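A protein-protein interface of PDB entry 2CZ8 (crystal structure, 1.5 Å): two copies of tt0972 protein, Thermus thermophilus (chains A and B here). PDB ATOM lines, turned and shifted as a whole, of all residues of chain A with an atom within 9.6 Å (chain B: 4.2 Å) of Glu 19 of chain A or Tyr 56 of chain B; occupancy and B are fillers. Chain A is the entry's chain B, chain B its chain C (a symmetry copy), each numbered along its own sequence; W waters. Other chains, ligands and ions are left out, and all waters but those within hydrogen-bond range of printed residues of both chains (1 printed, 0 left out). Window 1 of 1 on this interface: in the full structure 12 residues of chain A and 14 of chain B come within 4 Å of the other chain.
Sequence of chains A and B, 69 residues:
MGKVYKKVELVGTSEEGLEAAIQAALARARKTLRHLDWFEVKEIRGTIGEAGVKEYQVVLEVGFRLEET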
ATOM      1  N   GLY A  12     -19.446 -28.624  -2.667  1.00  0.00           N
ATOM      2  CA  GLY A  12     -18.214 -29.388  -2.610  1.00  0.00           C
ATOM      3  C   GLY A  12     -17.975 -29.826  -1.178  1.00  0.00           C
ATOM      4  O   GLY A  12     -18.318 -29.107  -0.241  1.00  0.00           O
ATOM      5  N   THR A  13     -17.408 -31.013  -0.983  1.00  0.00           N
ATOM      6  CA  THR A  13     -17.137 -31.469   0.369  1.00  0.00           C
ATOM      7  C   THR A  13     -15.727 -32.011   0.468  1.00  0.00           C
ATOM      8  O   THR A  13     -15.134 -32.434  -0.528  1.00  0.00           O
ATOM      9  CB  THR A  13     -18.127 -32.573   0.842  1.00  0.00           C
ATOM     10  OG1 THR A  13     -17.772 -33.834   0.260  1.00  0.00           O
ATOM     11  CG2 THR A  13     -19.551 -32.216   0.453  1.00  0.00           C
ATOM     12  N   SER A  14     -15.196 -31.967   1.680  1.00  0.00           N
ATOM     13  CA  SER A  14     -13.860 -32.472   1.965  1.00  0.00           C
ATOM     14  C   SER A  14     -13.646 -32.549   3.464  1.00  0.00           C
ATOM     15  O   SER A  14     -14.148 -31.718   4.224  1.00  0.00           O
ATOM     16  CB  SER A  14     -12.797 -31.562   1.354  1.00  0.00           C
ATOM     17  OG  SER A  14     -11.496 -31.982   1.745  1.00  0.00           O
ATOM     18  N   GLU A  15     -12.901 -33.560   3.892  1.00  0.00           N
ATOM     19  CA  GLU A  15     -12.588 -33.722   5.303  1.00  0.00           C
ATOM     20  C   GLU A  15     -11.384 -32.843   5.648  1.00  0.00           C
ATOM     21  O   GLU A  15     -11.096 -32.608   6.821  1.00  0.00           O
ATOM     22  CB  GLU A  15     -12.242 -35.183   5.617  1.00  0.00           C
ATOM     23  CG  GLU A  15     -13.403 -36.154   5.484  1.00  0.00           C
ATOM     24  CD  GLU A  15     -13.076 -37.548   5.998  1.00  0.00           C
ATOM     25  OE1 GLU A  15     -12.468 -37.658   7.084  1.00  0.00           O
ATOM     26  OE2 GLU A  15     -13.437 -38.534   5.322  1.00  0.00           O
ATOM     27  N   GLU A  16     -10.706 -32.344   4.617  1.00  0.00           N
ATOM     28  CA  GLU A  16      -9.502 -31.535   4.796  1.00  0.00           C
ATOM     29  C   GLU A  16      -9.717 -30.074   5.182  1.00  0.00           C
ATOM     30  O   GLU A  16      -9.113 -29.582   6.137  1.00  0.00           O
ATOM     31  CB  GLU A  16      -8.649 -31.594   3.523  1.00  0.00           C
ATOM     32  CG  GLU A  16      -8.307 -33.002   3.048  1.00  0.00           C
ATOM     33  CD  GLU A  16      -7.421 -33.000   1.814  1.00  0.00           C
ATOM     34  OE1 GLU A  16      -6.291 -32.475   1.897  1.00  0.00           O
ATOM     35  OE2 GLU A  16      -7.853 -33.519   0.761  1.00  0.00           O
ATOM     36  N   GLY A  17     -10.567 -29.375   4.440  1.00  0.00           N
ATOM     37  CA  GLY A  17     -10.802 -27.974   4.736  1.00  0.00           C
ATOM     38  C   GLY A  17     -11.686 -27.300   3.708  1.00  0.00           C
ATOM     39  O   GLY A  17     -12.208 -27.953   2.805  1.00  0.00           O
ATOM     40  N   LEU A  18     -11.830 -25.985   3.845  1.00  0.00           N
ATOM     41  CA  LEU A  18     -12.671 -25.181   2.963  1.00  0.00           C
ATOM     42  C   LEU A  18     -12.187 -25.117   1.516  1.00  0.00           C
ATOM     43  O   LEU A  18     -12.970 -25.315   0.581  1.00  0.00           O
ATOM     44  CB  LEU A  18     -12.800 -23.765   3.536  1.00  0.00           C
ATOM     45  CG  LEU A  18     -13.389 -23.712   4.947  1.00  0.00           C
ATOM     46  CD1 LEU A  18     -13.376 -22.271   5.446  1.00  0.00           C
ATOM     47  CD2 LEU A  18     -14.814 -24.269   4.946  1.00  0.00           C
ATOM     48  N   GLU A  19     -10.901 -24.833   1.328  1.00  0.00           N
ATOM     49  CA  GLU A  19     -10.343 -24.758  -0.014  1.00  0.00           C
ATOM     50  C   GLU A  19     -10.474 -26.100  -0.738  1.00  0.00           C
ATOM     51  O   GLU A  19     -10.814 -26.150  -1.926  1.00  0.00           O
ATOM     52  CB  GLU A  19      -8.867 -24.340   0.042  1.00  0.00           C
ATOM     53  CG  GLU A  19      -8.636 -22.846   0.258  1.00  0.00           C
ATOM     54  CD  GLU A  19      -8.698 -22.416   1.723  1.00  0.00           C
ATOM     55  OE1 GLU A  19      -9.223 -23.172   2.567  1.00  0.00           O
ATOM     56  OE2 GLU A  19      -8.223 -21.301   2.032  1.00  0.00           O
ATOM     57  N   ALA A  20     -10.200 -27.186  -0.026  1.00  0.00           N
ATOM     58  CA  ALA A  20     -10.302 -28.509  -0.620  1.00  0.00           C
ATOM     59  C   ALA A  20     -11.740 -28.793  -1.047  1.00  0.00           C
ATOM     60  O   ALA A  20     -11.972 -29.396  -2.099  1.00  0.00           O
ATOM     61  CB  ALA A  20      -9.817 -29.573   0.371  1.00  0.00           C
ATOM     62  N   ALA A  21     -12.703 -28.361  -0.233  1.00  0.00           N
ATOM     63  CA  ALA A  21     -14.109 -28.576  -0.566  1.00  0.00           C
ATOM     64  C   ALA A  21     -14.463 -27.807  -1.842  1.00  0.00           C
ATOM     65  O   ALA A  21     -15.169 -28.315  -2.719  1.00  0.00           O
ATOM     66  CB  ALA A  21     -14.994 -28.134   0.588  1.00  0.00           C
ATOM     67  N   ILE A  22     -13.982 -26.572  -1.940  1.00  0.00           N
ATOM     68  CA  ILE A  22     -14.236 -25.769  -3.128  1.00  0.00           C
ATOM     69  C   ILE A  22     -13.593 -26.429  -4.351  1.00  0.00           C
ATOM     70  O   ILE A  22     -14.211 -26.530  -5.407  1.00  0.00           O
ATOM     71  CB  ILE A  22     -13.684 -24.338  -2.942  1.00  0.00           C
ATOM     72  CG1 ILE A  22     -14.549 -23.600  -1.919  1.00  0.00           C
ATOM     73  CG2 ILE A  22     -13.670 -23.586  -4.273  1.00  0.00           C
ATOM     74  CD1 ILE A  22     -13.995 -22.247  -1.511  1.00  0.00           C
ATOM     75  N   GLN A  23     -12.353 -26.884  -4.204  1.00  0.00           N
ATOM     76  CA  GLN A  23     -11.668 -27.534  -5.315  1.00  0.00           C
ATOM     77  C   GLN A  23     -12.436 -28.767  -5.791  1.00  0.00           C
ATOM     78  O   GLN A  23     -12.489 -29.052  -6.991  1.00  0.00           O
ATOM     79  CB  GLN A  23     -10.245 -27.938  -4.905  1.00  0.00           C
ATOM     80  CG  GLN A  23      -9.291 -26.765  -4.709  1.00  0.00           C
ATOM     81  CD  GLN A  23      -8.857 -26.125  -6.013  1.00  0.00           C
ATOM     82  OE1 GLN A  23      -8.872 -24.906  -6.148  1.00  0.00           O
ATOM     83  NE2 GLN A  23      -8.450 -26.947  -6.977  1.00  0.00           N
ATOM     84  N   ALA A  24     -13.031 -29.499  -4.852  1.00  0.00           N
ATOM     85  CA  ALA A  24     -13.784 -30.698  -5.212  1.00  0.00           C
ATOM     86  C   ALA A  24     -14.971 -30.349  -6.109  1.00  0.00           C
ATOM     87  O   ALA A  24     -15.233 -31.027  -7.105  1.00  0.00           O
ATOM     88  CB  ALA A  24     -14.260 -31.417  -3.951  1.00  0.00           C
ATOM     89  N   ALA A  25     -15.693 -29.289  -5.758  1.00  0.00           N
ATOM     90  CA  ALA A  25     -16.839 -28.882  -6.561  1.00  0.00           C
ATOM     91  C   ALA A  25     -16.407 -28.410  -7.948  1.00  0.00           C
ATOM     92  O   ALA A  25     -17.045 -28.741  -8.947  1.00  0.00           O
ATOM     93  CB  ALA A  25     -17.612 -27.774  -5.849  1.00  0.00           C
ATOM     94  N   LEU A  26     -15.327 -27.637  -8.014  1.00  0.00           N
ATOM     95  CA  LEU A  26     -14.869 -27.137  -9.304  1.00  0.00           C
ATOM     96  C   LEU A  26     -14.366 -28.268 -10.193  1.00  0.00           C
ATOM     97  O   LEU A  26     -14.579 -28.248 -11.402  1.00  0.00           O
ATOM     98  CB  LEU A  26     -13.777 -26.079  -9.115  1.00  0.00           C
ATOM     99  CG  LEU A  26     -14.191 -24.838  -8.312  1.00  0.00           C
ATOM    100  CD1 LEU A  26     -13.014 -23.871  -8.221  1.00  0.00           C
ATOM    101  CD2 LEU A  26     -15.389 -24.166  -8.958  1.00  0.00           C
ATOM    102  N   ALA A  27     -13.710 -29.258  -9.594  1.00  0.00           N
ATOM    103  CA  ALA A  27     -13.204 -30.382 -10.372  1.00  0.00           C
ATOM    104  C   ALA A  27     -14.355 -31.159 -11.005  1.00  0.00           C
ATOM    105  O   ALA A  27     -14.255 -31.608 -12.148  1.00  0.00           O
ATOM    106  CB  ALA A  27     -12.376 -31.299  -9.491  1.00  0.00           C
ATOM    107  N   PHE A  39     -16.896 -18.220  -9.263  1.00  0.00           N
ATOM    108  CA  PHE A  39     -17.729 -18.901  -8.289  1.00  0.00           C
ATOM    109  C   PHE A  39     -18.066 -17.935  -7.170  1.00  0.00           C
ATOM    110  O   PHE A  39     -17.395 -16.914  -6.982  1.00  0.00           O
ATOM    111  CB  PHE A  39     -17.037 -20.154  -7.736  1.00  0.00           C
ATOM    112  CG  PHE A  39     -15.809 -19.869  -6.930  1.00  0.00           C
ATOM    113  CD1 PHE A  39     -15.892 -19.662  -5.557  1.00  0.00           C
ATOM    114  CD2 PHE A  39     -14.565 -19.801  -7.547  1.00  0.00           C
ATOM    115  CE1 PHE A  39     -14.744 -19.393  -4.803  1.00  0.00           C
ATOM    116  CE2 PHE A  39     -13.414 -19.532  -6.807  1.00  0.00           C
ATOM    117  CZ  PHE A  39     -13.505 -19.327  -5.431  1.00  0.00           C
ATOM    118  N   VAL A  41     -19.419 -18.207  -3.028  1.00  0.00           N
ATOM    119  CA  VAL A  41     -19.767 -19.066  -1.912  1.00  0.00           C
ATOM    120  C   VAL A  41     -21.093 -18.593  -1.333  1.00  0.00           C
ATOM    121  O   VAL A  41     -21.253 -17.416  -0.993  1.00  0.00           O
ATOM    122  CB  VAL A  41     -18.676 -19.049  -0.817  1.00  0.00           C
ATOM    123  CG1 VAL A  41     -19.164 -19.816   0.410  1.00  0.00           C
ATOM    124  CG2 VAL A  41     -17.397 -19.678  -1.354  1.00  0.00           C
ATOM    125  N   ILE A  44     -21.385 -22.065   4.085  1.00  0.00           N
ATOM    126  CA  ILE A  44     -20.325 -22.926   4.578  1.00  0.00           C
ATOM    127  C   ILE A  44     -20.979 -23.669   5.737  1.00  0.00           C
ATOM    128  O   ILE A  44     -21.540 -23.057   6.645  1.00  0.00           O
ATOM    129  CB  ILE A  44     -19.123 -22.137   5.109  1.00  0.00           C
ATOM    130  CG1 ILE A  44     -18.435 -21.407   3.957  1.00  0.00           C
ATOM    131  CG2 ILE A  44     -18.134 -23.091   5.783  1.00  0.00           C
ATOM    132  CD1 ILE A  44     -17.344 -20.459   4.401  1.00  0.00           C
ATOM    133  N   TYR A  56     -16.408 -30.929   5.685  1.00  0.00           N
ATOM    134  CA  TYR A  56     -16.648 -29.512   5.425  1.00  0.00           C
ATOM    135  C   TYR A  56     -17.508 -29.503   4.165  1.00  0.00           C
ATOM    136  O   TYR A  56     -17.242 -30.261   3.232  1.00  0.00           O
ATOM    137  CB  TYR A  56     -15.352 -28.758   5.121  1.00  0.00           C
ATOM    138  CG  TYR A  56     -14.498 -28.474   6.323  1.00  0.00           C
ATOM    139  CD1 TYR A  56     -13.459 -29.329   6.682  1.00  0.00           C
ATOM    140  CD2 TYR A  56     -14.736 -27.354   7.114  1.00  0.00           C
ATOM    141  CE1 TYR A  56     -12.677 -29.069   7.807  1.00  0.00           C
ATOM    142  CE2 TYR A  56     -13.964 -27.087   8.234  1.00  0.00           C
ATOM    143  CZ  TYR A  56     -12.940 -27.947   8.573  1.00  0.00           C
ATOM    144  OH  TYR A  56     -12.183 -27.673   9.685  1.00  0.00           O
ATOM    145  N   GLN A  57     -18.525 -28.647   4.133  1.00  0.00           N
ATOM    146  CA  GLN A  57     -19.423 -28.559   2.985  1.00  0.00           C
ATOM    147  C   GLN A  57     -19.548 -27.110   2.547  1.00  0.00           C
ATOM    148  O   GLN A  57     -20.015 -26.259   3.308  1.00  0.00           O
ATOM    149  CB  GLN A  57     -20.802 -29.111   3.353  1.00  0.00           C
ATOM    150  CG  GLN A  57     -20.746 -30.519   3.922  1.00  0.00           C
ATOM    151  CD  GLN A  57     -22.072 -30.981   4.488  1.00  0.00           C
ATOM    152  OE1 GLN A  57     -22.855 -30.179   4.997  1.00  0.00           O
ATOM    153  NE2 GLN A  57     -22.318 -32.284   4.429  1.00  0.00           N
ATOM    154  N   VAL A  58     -19.118 -26.821   1.325  1.00  0.00           N
ATOM    155  CA  VAL A  58     -19.192 -25.466   0.809  1.00  0.00           C
ATOM    156  C   VAL A  58     -20.182 -25.396  -0.351  1.00  0.00           C
ATOM    157  O   VAL A  58     -19.979 -26.016  -1.403  1.00  0.00           O
ATOM    158  CB  VAL A  58     -17.803 -24.971   0.347  1.00  0.00           C
ATOM    159  CG1 VAL A  58     -17.902 -23.541  -0.167  1.00  0.00           C
ATOM    160  CG2 VAL A  58     -16.826 -25.044   1.508  1.00  0.00           C
ATOM    161  N   LEU A  60     -21.774 -23.540  -3.303  1.00  0.00           N
ATOM    162  CA  LEU A  60     -21.378 -22.440  -4.160  1.00  0.00           C
ATOM    163  C   LEU A  60     -22.086 -22.403  -5.489  1.00  0.00           C
ATOM    164  O   LEU A  60     -22.643 -23.398  -5.949  1.00  0.00           O
ATOM    165  CB  LEU A  60     -19.860 -22.460  -4.381  1.00  0.00           C
ATOM    166  CG  LEU A  60     -19.186 -23.754  -4.854  1.00  0.00           C
ATOM    167  CD1 LEU A  60     -19.754 -24.180  -6.192  1.00  0.00           C
ATOM    168  CD2 LEU A  60     -17.682 -23.548  -4.973  1.00  0.00           C
ATOM    169  N   GLY B  12     -10.041  -8.230  -0.860  1.00  0.00           N
ATOM    170  CA  GLY B  12      -8.690  -8.752  -0.881  1.00  0.00           C
ATOM    171  C   GLY B  12      -8.657  -9.943  -1.814  1.00  0.00           C
ATOM    172  O   GLY B  12      -9.615 -10.727  -1.862  1.00  0.00           O
ATOM    173  N   THR B  13      -7.588 -10.080  -2.588  1.00  0.00           N
ATOM    174  CA  THR B  13      -7.490 -11.225  -3.481  1.00  0.00           C
ATOM    175  C   THR B  13      -6.158 -11.912  -3.287  1.00  0.00           C
ATOM    176  O   THR B  13      -5.184 -11.305  -2.829  1.00  0.00           O
ATOM    177  CB  THR B  13      -7.652 -10.840  -4.979  1.00  0.00           C
ATOM    178  OG1 THR B  13      -6.436 -10.263  -5.473  1.00  0.00           O
ATOM    179  CG2 THR B  13      -8.806  -9.844  -5.160  1.00  0.00           C
ATOM    180  N   SER B  14      -6.134 -13.199  -3.603  1.00  0.00           N
ATOM    181  CA  SER B  14      -4.911 -13.985  -3.494  1.00  0.00           C
ATOM    182  C   SER B  14      -5.087 -15.307  -4.205  1.00  0.00           C
ATOM    183  O   SER B  14      -6.193 -15.835  -4.303  1.00  0.00           O
ATOM    184  CB  SER B  14      -4.556 -14.256  -2.033  1.00  0.00           C
ATOM    185  OG  SER B  14      -3.419 -15.116  -1.943  1.00  0.00           O
ATOM    186  N   GLY B  17      -5.129 -18.639  -1.030  1.00  0.00           N
ATOM    187  CA  GLY B  17      -6.259 -19.162  -0.289  1.00  0.00           C
ATOM    188  C   GLY B  17      -7.083 -18.073   0.367  1.00  0.00           C
ATOM    189  O   GLY B  17      -6.798 -16.882   0.202  1.00  0.00           O
ATOM    190  N   LEU B  18      -8.104 -18.477   1.114  1.00  0.00           N
ATOM    191  CA  LEU B  18      -8.998 -17.546   1.796  1.00  0.00           C
ATOM    192  C   LEU B  18      -8.295 -16.638   2.778  1.00  0.00           C
ATOM    193  O   LEU B  18      -8.438 -15.420   2.719  1.00  0.00           O
ATOM    194  CB  LEU B  18     -10.092 -18.310   2.541  1.00  0.00           C
ATOM    195  CG  LEU B  18     -11.049 -19.071   1.632  1.00  0.00           C
ATOM    196  CD1 LEU B  18     -11.996 -19.915   2.459  1.00  0.00           C
ATOM    197  CD2 LEU B  18     -11.811 -18.077   0.776  1.00  0.00           C
ATOM    198  N   GLU B  19      -7.558 -17.234   3.708  1.00  0.00           N
ATOM    199  CA  GLU B  19      -6.858 -16.439   4.692  1.00  0.00           C
ATOM    200  C   GLU B  19      -5.917 -15.446   4.008  1.00  0.00           C
ATOM    201  O   GLU B  19      -5.860 -14.277   4.398  1.00  0.00           O
ATOM    202  CB  GLU B  19      -6.094 -17.344   5.672  1.00  0.00           C
ATOM    203  CG  GLU B  19      -6.969 -17.922   6.796  1.00  0.00           C
ATOM    204  CD  GLU B  19      -7.609 -19.254   6.441  1.00  0.00           C
ATOM    205  OE1 GLU B  19      -7.735 -19.556   5.237  1.00  0.00           O
ATOM    206  OE2 GLU B  19      -8.002 -19.996   7.370  1.00  0.00           O
ATOM    207  N   ALA B  21      -6.206 -14.048   1.140  1.00  0.00           N
ATOM    208  CA  ALA B  21      -6.979 -12.976   0.519  1.00  0.00           C
ATOM    209  C   ALA B  21      -7.359 -11.953   1.581  1.00  0.00           C
ATOM    210  O   ALA B  21      -7.285 -10.742   1.353  1.00  0.00           O
ATOM    211  CB  ALA B  21      -8.222 -13.538  -0.131  1.00  0.00           C
ATOM    212  N   ARG B  45     -15.742 -15.210  -2.947  1.00  0.00           N
ATOM    213  CA  ARG B  45     -15.954 -15.608  -4.327  1.00  0.00           C
ATOM    214  C   ARG B  45     -14.601 -15.742  -4.982  1.00  0.00           C
ATOM    215  O   ARG B  45     -13.576 -15.717  -4.297  1.00  0.00           O
ATOM    216  CB  ARG B  45     -16.818 -14.572  -5.050  1.00  0.00           C
ATOM    217  CG  ARG B  45     -16.351 -13.132  -4.928  1.00  0.00           C
ATOM    218  CD  ARG B  45     -17.516 -12.170  -5.205  1.00  0.00           C
ATOM    219  NE  ARG B  45     -18.142 -12.417  -6.503  1.00  0.00           N
ATOM    220  CZ  ARG B  45     -19.344 -11.973  -6.864  1.00  0.00           C
ATOM    221  NH1 ARG B  45     -20.071 -11.249  -6.023  1.00  0.00           N
ATOM    222  NH2 ARG B  45     -19.824 -12.261  -8.070  1.00  0.00           N
ATOM    223  N   VAL B  53      -9.507 -23.179  -8.520  1.00  0.00           N
ATOM    224  CA  VAL B  53      -9.586 -21.761  -8.193  1.00  0.00           C
ATOM    225  C   VAL B  53      -8.360 -21.050  -8.740  1.00  0.00           C
ATOM    226  O   VAL B  53      -7.232 -21.517  -8.566  1.00  0.00           O
ATOM    227  CB  VAL B  53      -9.612 -21.502  -6.666  1.00  0.00           C
ATOM    228  CG1 VAL B  53      -9.592 -19.996  -6.397  1.00  0.00           C
ATOM    229  CG2 VAL B  53     -10.846 -22.134  -6.042  1.00  0.00           C
ATOM    230  N   GLU B  55      -8.132 -17.237  -8.572  1.00  0.00           N
ATOM    231  CA  GLU B  55      -7.942 -16.206  -7.568  1.00  0.00           C
ATOM    232  C   GLU B  55      -9.087 -16.185  -6.560  1.00  0.00           C
ATOM    233  O   GLU B  55     -10.257 -16.168  -6.950  1.00  0.00           O
ATOM    234  CB  GLU B  55      -7.841 -14.849  -8.279  1.00  0.00           C
ATOM    235  CG  GLU B  55      -7.728 -13.625  -7.399  1.00  0.00           C
ATOM    236  CD  GLU B  55      -7.720 -12.341  -8.219  1.00  0.00           C
ATOM    237  OE1 GLU B  55      -6.694 -12.046  -8.872  1.00  0.00           O
ATOM    238  OE2 GLU B  55      -8.747 -11.632  -8.227  1.00  0.00           O
ATOM    239  N   TYR B  56      -8.756 -16.231  -5.273  1.00  0.00           N
ATOM    240  CA  TYR B  56      -9.778 -16.126  -4.235  1.00  0.00           C
ATOM    241  C   TYR B  56     -10.013 -14.639  -4.041  1.00  0.00           C
ATOM    242  O   TYR B  56      -9.071 -13.839  -4.082  1.00  0.00           O
ATOM    243  CB  TYR B  56      -9.315 -16.720  -2.900  1.00  0.00           C
ATOM    244  CG  TYR B  56      -9.184 -18.225  -2.896  1.00  0.00           C
ATOM    245  CD1 TYR B  56      -7.986 -18.831  -3.261  1.00  0.00           C
ATOM    246  CD2 TYR B  56     -10.260 -19.040  -2.538  1.00  0.00           C
ATOM    247  CE1 TYR B  56      -7.851 -20.213  -3.269  1.00  0.00           C
ATOM    248  CE2 TYR B  56     -10.135 -20.431  -2.545  1.00  0.00           C
ATOM    249  CZ  TYR B  56      -8.926 -21.003  -2.912  1.00  0.00           C
ATOM    250  OH  TYR B  56      -8.783 -22.375  -2.925  1.00  0.00           O
ATOM    251  N   GLN B  57     -11.268 -14.269  -3.824  1.00  0.00           N
ATOM    252  CA  GLN B  57     -11.624 -12.867  -3.627  1.00  0.00           C
ATOM    253  C   GLN B  57     -12.535 -12.768  -2.413  1.00  0.00           C
ATOM    254  O   GLN B  57     -13.634 -13.323  -2.406  1.00  0.00           O
ATOM    255  CB  GLN B  57     -12.334 -12.336  -4.873  1.00  0.00           C
ATOM    256  CG  GLN B  57     -11.510 -12.496  -6.148  1.00  0.00           C
ATOM    257  CD  GLN B  57     -12.311 -12.249  -7.407  1.00  0.00           C
ATOM    258  OE1 GLN B  57     -13.525 -12.451  -7.427  1.00  0.00           O
ATOM    259  NE2 GLN B  57     -11.633 -11.838  -8.474  1.00  0.00           N
HETATM  260  O   HOH W   1      -5.928 -20.923   3.698  1.00  0.00           O
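O of Ser 14 of chain B lies within hydrogen-bond range of N of Tyr 56 of chain B.
The backbone carbonyl oxygen (O) of Arg 45 of chain B is in hydrogen-bond range of the backbone NH (N) of Gln 57 of chain B, 2.8 Å away.
OE2 of Glu 19 of chain A touches CA of Gly 17 of chain B, 3.7 Å away.
OE2 of Glu 19 of chain A touches OE1 of Glu 19 of chain B (3.7 Å).
Glu 19 of chain A touches Tyr 56 of chain B.
Val 53 of chain B touches Ile 22 of chain A.
Leu 26 of chain A touches Val 53 of chain B (CD1 to CG2, 3.5 Å).
Phe 39 of chain A touches Arg 45 of chain B.
Phe 39 of chain A touches Val 53 of chain B (CE2 to CG2, 3.7 Å).
Printed residues of chain B that touch a printed residue of chain A: Gly 17, Leu 18, Glu 19, Arg 45, Val 53 and Tyr 56.
Hydrophobic or aromatic side chains of chain B within 4 Å of the printed part of chain A: Leu 18, Val 53 and Tyr 56.
Along chain B the printed residues that touch a printed residue of chain A span positions 17 to 56.
Among the printed residues, 9 pairs touch across the chains.
Glu 19 of chain A touches Gly 17 of chain B, but with the chains exchanged Gly 17 of chain A does not touch Glu 19 of chain B (8.8 Å).
Glu 19 of chain A touches Leu 18 of chain B, but with the chains exchanged Leu 18 of chain A does not touch Glu 19 of chain B (6.1 Å).
Glu 19 of chain B touches its own counterpart, Glu 19 of chain A.
Glu 19 of chain A touches Tyr 56 of chain B, but with the chains exchanged Tyr 56 of chain A does not touch Glu 19 of chain B (9.0 Å).
Positions printed for both chains: 12, 13, 14, 17, 18, 19, 21, 56 and 57.
OE2 of Glu 19 of chain A sits at hydrogen-bond distance from N of Leu 18 of chain B (3.0 Å).
The side-chain amide oxygen (OE1) of Gln 23 of chain A sits at hydrogen-bond distance from the backbone NH (N) of Val 53 of chain B (3.0 Å).
Printed residues of chain B within 4 Å of Glu 19 of chain A: Gly 17 (3.7 Å), Leu 18 (3.0 Å), Glu 19 (3.7 Å) and Tyr 56 (3.2 Å).
Of the printed residues of chain A, Tyr 56 of chain B touches Glu 19 (3.2 Å).
No residue of chain A comes within 4 Å of Thr 13 of chain B.
No residue of chain A comes within 4 Å of Gln 57 of chain B.
Printed residues of chain A within 4 Å of Val 53 of chain B: Ile 22 (3.6 Å), Gln 23 (3.0 Å), Leu 26 (3.5 Å) and Phe 39 (3.7 Å).
Printed residues of chain A within 4 Å of Gly 17 of chain B: Glu 19 (3.7 Å).
Of the printed residues of chain B, Leu 26 of chain A touches Val 53 (3.5 Å).
Water W1 bridges the side-chain carboxylate (OE1) of Glu 19 of chain B (2.7 Å) and the side-chain carboxylate (OE2) of Glu 19 of chain A (2.9 Å).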
